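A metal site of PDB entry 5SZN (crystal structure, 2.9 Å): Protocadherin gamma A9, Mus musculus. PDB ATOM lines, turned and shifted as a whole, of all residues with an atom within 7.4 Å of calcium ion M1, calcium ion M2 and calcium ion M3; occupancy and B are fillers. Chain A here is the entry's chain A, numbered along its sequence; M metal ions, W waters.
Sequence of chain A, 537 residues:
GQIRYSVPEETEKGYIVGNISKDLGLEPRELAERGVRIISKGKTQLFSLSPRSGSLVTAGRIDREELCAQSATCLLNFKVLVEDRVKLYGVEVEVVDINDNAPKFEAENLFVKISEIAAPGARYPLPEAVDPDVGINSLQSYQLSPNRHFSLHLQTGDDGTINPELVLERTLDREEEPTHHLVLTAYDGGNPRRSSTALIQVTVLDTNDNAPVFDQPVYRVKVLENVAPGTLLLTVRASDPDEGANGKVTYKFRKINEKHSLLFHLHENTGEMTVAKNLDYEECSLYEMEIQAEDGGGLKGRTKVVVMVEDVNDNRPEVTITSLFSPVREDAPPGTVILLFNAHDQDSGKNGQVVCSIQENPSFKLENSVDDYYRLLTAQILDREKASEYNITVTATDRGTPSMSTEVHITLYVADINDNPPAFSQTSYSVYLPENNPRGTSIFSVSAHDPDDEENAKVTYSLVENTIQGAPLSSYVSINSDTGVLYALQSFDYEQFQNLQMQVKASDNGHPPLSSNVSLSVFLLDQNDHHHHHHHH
OD1 of Asn 210 lies close to OE2 of Glu 175 (3.3 Å).
The guanidinium group (NH1) of Arg 174 sits close to the side-chain carboxylate (OE2) of Glu 175 (2.8 Å).
The side-chain amide oxygen of Asn 210 lies close to the side-chain carboxylate of Asp 209.
N of Leu 299 lies within hydrogen-bond range of OD1 of Asp 295 (3.3 Å).
The side-chain carboxylate (OD1) of Asp 295 lies close to the backbone NH (N) of Gly 297 (3.3 Å).
The side-chain carboxylate of Asp 206 sits at hydrogen-bond distance from the backbone NH of Glu 243.
O of Pro 241 lies within hydrogen-bond range of NH1 of Arg 174 (3.1 Å).
The guanidinium group of Arg 174 lies within salt-bridge range of the side-chain carboxylate of Glu 243 (3.4 Å).
Merely in contact with calcium ion M1: Arg 174 (3.8 Å).
Within 4 Å of calcium ion M1: Glu 116, Arg 174, Glu 175, Asp 206, Thr 207, Asp 209, Asn 210 and Asp 242.
Within 4 Å of calcium ion M2: Glu 116, Asp 173, Glu 175, Asp 209 and Asn 210.
Within 4 Å of calcium ion M3: Asn 208, Asn 210, Asp 240, Asp 242, Asn 246 and Asp 295.
The side-chain carboxylate (OE2) of Glu 175 is bound to calcium ion M1.
Calcium ion M1 is bound by the side-chain carboxylate (OE1) of Glu 116, at 2.5 Å.
The side-chain carboxylate (OD1) of Asp 209 is bound to calcium ion M1.
OD1 of Asp 242 binds calcium ion M1 (2.7 Å).
O of Thr 207 is bound to calcium ion M1 (2.7 Å).
The side-chain carboxylate (OD1) of Asp 206 binds calcium ion M1.
Calcium ion M1 is bound by OE1 of Glu 175 (2.9 Å).
The side-chain carboxylate (OE2) of Glu 116 binds calcium ion M2.
Calcium ion M2 is bound by OD1 of Asp 173 (2.4 Å).
Calcium ion M2 is bound by the side-chain carboxylate (OE1) of Glu 175 (2.5 Å).
OD2 of Asp 209 is bound to calcium ion M2, 2.6 Å away.
Calcium ion M3 is bound by OD2 of Asp 242 (2.2 Å), O of Asn 210 (2.4 Å), O of Asn 246 (2.4 Å), OD1 of Asn 208 (2.4 Å), OD2 of Asp 295 (2.6 Å), OD1 of Asp 240 (2.7 Å) and OD2 of Asp 240 (2.7 Å).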
ATOM      1  N   GLU A 116      32.916  12.281  25.225  1.00  0.00           N
ATOM      2  CA  GLU A 116      33.041  12.487  23.784  1.00  0.00           C
ATOM      3  C   GLU A 116      33.884  13.724  23.477  1.00  0.00           C
ATOM      4  O   GLU A 116      34.533  13.785  22.426  1.00  0.00           O
ATOM      5  CB  GLU A 116      31.650  12.610  23.164  1.00  0.00           C
ATOM      6  CG  GLU A 116      31.623  12.672  21.649  1.00  0.00           C
ATOM      7  CD  GLU A 116      30.205  12.830  21.120  1.00  0.00           C
ATOM      8  OE1 GLU A 116      29.255  12.709  21.922  1.00  0.00           O
ATOM      9  OE2 GLU A 116      30.054  13.085  19.904  1.00  0.00           O
ATOM     10  N   LEU A 172      37.153  10.420  20.542  1.00  0.00           N
ATOM     11  CA  LEU A 172      36.087   9.429  20.526  1.00  0.00           C
ATOM     12  C   LEU A 172      34.775  10.057  20.057  1.00  0.00           C
ATOM     13  O   LEU A 172      34.589  11.274  20.076  1.00  0.00           O
ATOM     14  CB  LEU A 172      35.894   8.812  21.904  1.00  0.00           C
ATOM     15  CG  LEU A 172      37.040   7.896  22.370  1.00  0.00           C
ATOM     16  CD1 LEU A 172      36.670   7.202  23.665  1.00  0.00           C
ATOM     17  CD2 LEU A 172      37.370   6.873  21.287  1.00  0.00           C
ATOM     18  N   ASP A 173      33.868   9.192  19.606  1.00  0.00           N
ATOM     19  CA  ASP A 173      32.534   9.625  19.174  1.00  0.00           C
ATOM     20  C   ASP A 173      31.549   8.530  19.525  1.00  0.00           C
ATOM     21  O   ASP A 173      31.648   7.408  19.021  1.00  0.00           O
ATOM     22  CB  ASP A 173      32.503   9.909  17.667  1.00  0.00           C
ATOM     23  CG  ASP A 173      31.216  10.554  17.228  1.00  0.00           C
ATOM     24  OD1 ASP A 173      30.740  11.483  17.917  1.00  0.00           O
ATOM     25  OD2 ASP A 173      30.660  10.134  16.188  1.00  0.00           O
ATOM     26  N   ARG A 174      30.591   8.848  20.407  1.00  0.00           N
ATOM     27  CA  ARG A 174      29.621   7.858  20.837  1.00  0.00           C
ATOM     28  C   ARG A 174      28.561   7.585  19.766  1.00  0.00           C
ATOM     29  O   ARG A 174      27.940   6.523  19.796  1.00  0.00           O
ATOM     30  CB  ARG A 174      28.931   8.319  22.116  1.00  0.00           C
ATOM     31  CG  ARG A 174      28.101   9.563  21.936  1.00  0.00           C
ATOM     32  CD  ARG A 174      27.139   9.772  23.089  1.00  0.00           C
ATOM     33  NE  ARG A 174      26.184   8.678  23.218  1.00  0.00           N
ATOM     34  CZ  ARG A 174      25.016   8.622  22.588  1.00  0.00           C
ATOM     35  NH1 ARG A 174      24.664   9.593  21.759  1.00  0.00           N
ATOM     36  NH2 ARG A 174      24.213   7.588  22.770  1.00  0.00           N
ATOM     37  N   GLU A 175      28.358   8.522  18.836  1.00  0.00           N
ATOM     38  CA  GLU A 175      27.313   8.353  17.843  1.00  0.00           C
ATOM     39  C   GLU A 175      27.648   7.232  16.860  1.00  0.00           C
ATOM     40  O   GLU A 175      26.747   6.604  16.301  1.00  0.00           O
ATOM     41  CB  GLU A 175      27.084   9.659  17.085  1.00  0.00           C
ATOM     42  CG  GLU A 175      26.252  10.669  17.857  1.00  0.00           C
ATOM     43  CD  GLU A 175      26.917  11.139  19.128  1.00  0.00           C
ATOM     44  OE1 GLU A 175      28.149  11.357  19.112  1.00  0.00           O
ATOM     45  OE2 GLU A 175      26.227  11.280  20.158  1.00  0.00           O
ATOM     46  N   GLU A 176      28.936   6.964  16.654  1.00  0.00           N
ATOM     47  CA  GLU A 176      29.354   5.872  15.785  1.00  0.00           C
ATOM     48  C   GLU A 176      29.481   4.564  16.548  1.00  0.00           C
ATOM     49  O   GLU A 176      29.066   3.505  16.055  1.00  0.00           O
ATOM     50  CB  GLU A 176      30.687   6.216  15.116  1.00  0.00           C
ATOM     51  CG  GLU A 176      30.733   7.610  14.503  1.00  0.00           C
ATOM     52  CD  GLU A 176      32.100   7.968  13.946  1.00  0.00           C
ATOM     53  OE1 GLU A 176      32.899   7.041  13.697  1.00  0.00           O
ATOM     54  OE2 GLU A 176      32.365   9.169  13.769  1.00  0.00           O
ATOM     55  N   LEU A 205      31.016   8.832  27.124  1.00  0.00           N
ATOM     56  CA  LEU A 205      29.956   9.696  27.627  1.00  0.00           C
ATOM     57  C   LEU A 205      29.318  10.457  26.462  1.00  0.00           C
ATOM     58  O   LEU A 205      29.702  10.310  25.296  1.00  0.00           O
ATOM     59  CB  LEU A 205      30.493  10.653  28.691  1.00  0.00           C
ATOM     60  CG  LEU A 205      31.025  10.005  29.968  1.00  0.00           C
ATOM     61  CD1 LEU A 205      31.355  11.072  31.008  1.00  0.00           C
ATOM     62  CD2 LEU A 205      30.041   8.989  30.522  1.00  0.00           C
ATOM     63  N   ASP A 206      28.332  11.288  26.776  1.00  0.00           N
ATOM     64  CA  ASP A 206      27.555  11.984  25.769  1.00  0.00           C
ATOM     65  C   ASP A 206      27.781  13.491  25.888  1.00  0.00           C
ATOM     66  O   ASP A 206      27.576  14.073  26.957  1.00  0.00           O
ATOM     67  CB  ASP A 206      26.063  11.670  25.889  1.00  0.00           C
ATOM     68  CG  ASP A 206      25.248  12.247  24.742  1.00  0.00           C
ATOM     69  OD1 ASP A 206      25.850  12.596  23.708  1.00  0.00           O
ATOM     70  OD2 ASP A 206      24.008  12.329  24.873  1.00  0.00           O
ATOM     71  N   THR A 207      28.209  14.102  24.790  1.00  0.00           N
ATOM     72  CA  THR A 207      28.288  15.550  24.665  1.00  0.00           C
ATOM     73  C   THR A 207      27.222  16.006  23.677  1.00  0.00           C
ATOM     74  O   THR A 207      27.010  15.370  22.639  1.00  0.00           O
ATOM     75  CB  THR A 207      29.679  15.994  24.179  1.00  0.00           C
ATOM     76  OG1 THR A 207      30.675  15.578  25.120  1.00  0.00           O
ATOM     77  CG2 THR A 207      29.730  17.513  24.026  1.00  0.00           C
ATOM     78  N   ASN A 208      26.542  17.099  24.005  1.00  0.00           N
ATOM     79  CA  ASN A 208      25.513  17.653  23.131  1.00  0.00           C
ATOM     80  C   ASN A 208      26.208  18.354  21.956  1.00  0.00           C
ATOM     81  O   ASN A 208      26.322  19.576  21.898  1.00  0.00           O
ATOM     82  CB  ASN A 208      24.606  18.605  23.907  1.00  0.00           C
ATOM     83  CG  ASN A 208      23.369  18.991  23.127  1.00  0.00           C
ATOM     84  OD1 ASN A 208      23.059  18.398  22.093  1.00  0.00           O
ATOM     85  ND2 ASN A 208      22.635  19.982  23.632  1.00  0.00           N
ATOM     86  N   ASP A 209      26.677  17.539  21.022  1.00  0.00           N
ATOM     87  CA  ASP A 209      27.320  18.035  19.804  1.00  0.00           C
ATOM     88  C   ASP A 209      26.511  17.700  18.554  1.00  0.00           C
ATOM     89  O   ASP A 209      26.991  17.922  17.432  1.00  0.00           O
ATOM     90  CB  ASP A 209      28.741  17.482  19.688  1.00  0.00           C
ATOM     91  CG  ASP A 209      28.787  15.972  19.668  1.00  0.00           C
ATOM     92  OD1 ASP A 209      27.777  15.337  20.003  1.00  0.00           O
ATOM     93  OD2 ASP A 209      29.853  15.419  19.325  1.00  0.00           O
ATOM     94  N   ASN A 210      25.297  17.163  18.712  1.00  0.00           N
ATOM     95  CA  ASN A 210      24.407  16.859  17.609  1.00  0.00           C
ATOM     96  C   ASN A 210      23.216  17.809  17.656  1.00  0.00           C
ATOM     97  O   ASN A 210      22.428  17.781  18.602  1.00  0.00           O
ATOM     98  CB  ASN A 210      23.924  15.405  17.667  1.00  0.00           C
ATOM     99  CG  ASN A 210      25.026  14.418  17.387  1.00  0.00           C
ATOM    100  OD1 ASN A 210      25.659  13.891  18.307  1.00  0.00           O
ATOM    101  ND2 ASN A 210      25.267  14.149  16.107  1.00  0.00           N
ATOM    102  N   ALA A 211      23.093  18.651  16.615  1.00  0.00           N
ATOM    103  CA  ALA A 211      21.935  19.518  16.513  1.00  0.00           C
ATOM    104  C   ALA A 211      20.797  18.813  15.792  1.00  0.00           C
ATOM    105  O   ALA A 211      21.038  17.942  14.945  1.00  0.00           O
ATOM    106  CB  ALA A 211      22.297  20.802  15.766  1.00  0.00           C
ATOM    107  N   PRO A 212      19.548  19.142  16.112  1.00  0.00           N
ATOM    108  CA  PRO A 212      18.427  18.510  15.407  1.00  0.00           C
ATOM    109  C   PRO A 212      18.438  18.859  13.928  1.00  0.00           C
ATOM    110  O   PRO A 212      18.658  20.013  13.546  1.00  0.00           O
ATOM    111  CB  PRO A 212      17.196  19.095  16.112  1.00  0.00           C
ATOM    112  CG  PRO A 212      17.691  19.555  17.446  1.00  0.00           C
ATOM    113  CD  PRO A 212      19.098  20.014  17.206  1.00  0.00           C
ATOM    114  N   SER A 239      15.935  14.746  13.685  1.00  0.00           N
ATOM    115  CA  SER A 239      16.904  13.728  14.073  1.00  0.00           C
ATOM    116  C   SER A 239      17.866  14.307  15.104  1.00  0.00           C
ATOM    117  O   SER A 239      18.511  15.323  14.852  1.00  0.00           O
ATOM    118  CB  SER A 239      17.667  13.198  12.863  1.00  0.00           C
ATOM    119  OG  SER A 239      16.800  12.607  11.921  1.00  0.00           O
ATOM    120  N   ASP A 240      17.939  13.659  16.265  1.00  0.00           N
ATOM    121  CA  ASP A 240      18.920  14.015  17.294  1.00  0.00           C
ATOM    122  C   ASP A 240      19.486  12.723  17.872  1.00  0.00           C
ATOM    123  O   ASP A 240      18.880  12.120  18.784  1.00  0.00           O
ATOM    124  CB  ASP A 240      18.296  14.875  18.388  1.00  0.00           C
ATOM    125  CG  ASP A 240      19.334  15.695  19.145  1.00  0.00           C
ATOM    126  OD1 ASP A 240      20.529  15.344  19.080  1.00  0.00           O
ATOM    127  OD2 ASP A 240      18.947  16.687  19.796  1.00  0.00           O
ATOM    128  N   PRO A 241      20.634  12.262  17.372  1.00  0.00           N
ATOM    129  CA  PRO A 241      21.205  10.999  17.860  1.00  0.00           C
ATOM    130  C   PRO A 241      21.772  11.071  19.272  1.00  0.00           C
ATOM    131  O   PRO A 241      22.274  10.052  19.760  1.00  0.00           O
ATOM    132  CB  PRO A 241      22.324  10.704  16.847  1.00  0.00           C
ATOM    133  CG  PRO A 241      22.026  11.584  15.669  1.00  0.00           C
ATOM    134  CD  PRO A 241      21.385  12.810  16.236  1.00  0.00           C
ATOM    135  N   ASP A 242      21.702  12.219  19.948  1.00  0.00           N
ATOM    136  CA  ASP A 242      22.218  12.333  21.298  1.00  0.00           C
ATOM    137  C   ASP A 242      21.397  11.483  22.263  1.00  0.00           C
ATOM    138  O   ASP A 242      20.451  10.785  21.879  1.00  0.00           O
ATOM    139  CB  ASP A 242      22.230  13.800  21.741  1.00  0.00           C
ATOM    140  CG  ASP A 242      23.310  14.601  21.060  1.00  0.00           C
ATOM    141  OD1 ASP A 242      24.426  14.072  20.880  1.00  0.00           O
ATOM    142  OD2 ASP A 242      23.051  15.769  20.699  1.00  0.00           O
ATOM    143  N   GLU A 243      21.760  11.552  23.534  1.00  0.00           N
ATOM    144  CA  GLU A 243      21.155  10.727  24.577  1.00  0.00           C
ATOM    145  C   GLU A 243      20.554  11.609  25.660  1.00  0.00           C
ATOM    146  O   GLU A 243      21.160  12.603  26.074  1.00  0.00           O
ATOM    147  CB  GLU A 243      22.199   9.771  25.187  1.00  0.00           C
ATOM    148  CG  GLU A 243      21.622   8.784  26.189  1.00  0.00           C
ATOM    149  CD  GLU A 243      22.652   7.769  26.625  1.00  0.00           C
ATOM    150  OE1 GLU A 243      23.789   7.805  26.115  1.00  0.00           O
ATOM    151  OE2 GLU A 243      22.326   6.913  27.480  1.00  0.00           O
ATOM    152  N   ALA A 245      18.025  14.295  27.462  1.00  0.00           N
ATOM    153  CA  ALA A 245      17.412  15.554  27.058  1.00  0.00           C
ATOM    154  C   ALA A 245      18.078  16.134  25.825  1.00  0.00           C
ATOM    155  O   ALA A 245      17.450  16.886  25.073  1.00  0.00           O
ATOM    156  CB  ALA A 245      17.455  16.555  28.210  1.00  0.00           C
ATOM    157  N   ASN A 246      19.336  15.768  25.579  1.00  0.00           N
ATOM    158  CA  ASN A 246      20.023  16.220  24.381  1.00  0.00           C
ATOM    159  C   ASN A 246      19.506  15.535  23.130  1.00  0.00           C
ATOM    160  O   ASN A 246      19.884  15.936  22.029  1.00  0.00           O
ATOM    161  CB  ASN A 246      21.527  15.977  24.510  1.00  0.00           C
ATOM    162  CG  ASN A 246      22.122  16.672  25.722  1.00  0.00           C
ATOM    163  OD1 ASN A 246      21.608  17.698  26.181  1.00  0.00           O
ATOM    164  ND2 ASN A 246      23.215  16.132  26.230  1.00  0.00           N
ATOM    165  N   GLY A 247      18.661  14.510  23.261  1.00  0.00           N
ATOM    166  CA  GLY A 247      18.093  13.840  22.102  1.00  0.00           C
ATOM    167  C   GLY A 247      16.605  14.096  21.961  1.00  0.00           C
ATOM    168  O   GLY A 247      15.970  13.599  21.027  1.00  0.00           O
ATOM    169  N   LYS A 248      16.041  14.869  22.886  1.00  0.00           N
ATOM    170  CA  LYS A 248      14.626  15.224  22.849  1.00  0.00           C
ATOM    171  C   LYS A 248      14.399  16.387  21.902  1.00  0.00           C
ATOM    172  O   LYS A 248      15.285  17.209  21.673  1.00  0.00           O
ATOM    173  CB  LYS A 248      14.136  15.569  24.259  1.00  0.00           C
ATOM    174  CG  LYS A 248      12.650  15.813  24.371  1.00  0.00           C
ATOM    175  CD  LYS A 248      11.847  14.605  23.916  1.00  0.00           C
ATOM    176  CE  LYS A 248      10.380  14.948  23.751  1.00  0.00           C
ATOM    177  NZ  LYS A 248       9.814  15.531  25.010  1.00  0.00           N
ATOM    178  N   GLU A 294      14.164  22.188  18.884  1.00  0.00           N
ATOM    179  CA  GLU A 294      15.242  22.350  19.845  1.00  0.00           C
ATOM    180  C   GLU A 294      15.352  21.116  20.718  1.00  0.00           C
ATOM    181  O   GLU A 294      14.395  20.350  20.875  1.00  0.00           O
ATOM    182  CB  GLU A 294      15.042  23.594  20.720  1.00  0.00           C
ATOM    183  CG  GLU A 294      15.183  24.910  19.975  1.00  0.00           C
ATOM    184  CD  GLU A 294      14.950  26.116  20.859  1.00  0.00           C
ATOM    185  OE1 GLU A 294      15.133  25.995  22.093  1.00  0.00           O
ATOM    186  OE2 GLU A 294      14.576  27.184  20.330  1.00  0.00           O
ATOM    187  N   ASP A 295      16.529  20.925  21.300  1.00  0.00           N
ATOM    188  CA  ASP A 295      16.833  19.801  22.163  1.00  0.00           C
ATOM    189  C   ASP A 295      16.934  20.280  23.616  1.00  0.00           C
ATOM    190  O   ASP A 295      16.302  21.286  23.982  1.00  0.00           O
ATOM    191  CB  ASP A 295      18.088  19.108  21.646  1.00  0.00           C
ATOM    192  CG  ASP A 295      19.286  20.038  21.590  1.00  0.00           C
ATOM    193  OD1 ASP A 295      19.110  21.253  21.809  1.00  0.00           O
ATOM    194  OD2 ASP A 295      20.408  19.551  21.303  1.00  0.00           O
ATOM    195  N   GLY A 296      17.707  19.567  24.437  1.00  0.00           N
ATOM    196  CA  GLY A 296      17.898  20.003  25.812  1.00  0.00           C
ATOM    197  C   GLY A 296      18.667  21.305  25.905  1.00  0.00           C
ATOM    198  O   GLY A 296      18.323  22.178  26.716  1.00  0.00           O
ATOM    199  N   GLY A 297      19.712  21.457  25.098  1.00  0.00           N
ATOM    200  CA  GLY A 297      20.466  22.686  25.036  1.00  0.00           C
ATOM    201  C   GLY A 297      19.897  23.655  24.006  1.00  0.00           C
ATOM    202  O   GLY A 297      18.786  23.487  23.501  1.00  0.00           O
ATOM    203  N   LEU A 299      20.698  24.004  21.082  1.00  0.00           N
ATOM    204  CA  LEU A 299      20.871  23.508  19.724  1.00  0.00           C
ATOM    205  C   LEU A 299      19.513  23.445  19.023  1.00  0.00           C
ATOM    206  O   LEU A 299      18.538  22.924  19.583  1.00  0.00           O
ATOM    207  CB  LEU A 299      21.543  22.133  19.739  1.00  0.00           C
ATOM    208  CG  LEU A 299      23.048  22.062  19.990  1.00  0.00           C
ATOM    209  CD1 LEU A 299      23.388  22.388  21.435  1.00  0.00           C
ATOM    210  CD2 LEU A 299      23.591  20.690  19.622  1.00  0.00           C
HETATM  211 CA    CA M   1      26.938  13.074  21.182  1.00  0.00          CA
HETATM  212 CA    CA M   2      29.150  13.296  17.973  1.00  0.00          CA
HETATM  213 CA    CA M   3      21.400  17.252  20.702  1.00  0.00          CA
HETATM  214  O   HOH W   1      30.384  15.689  15.989  1.00  0.00           O
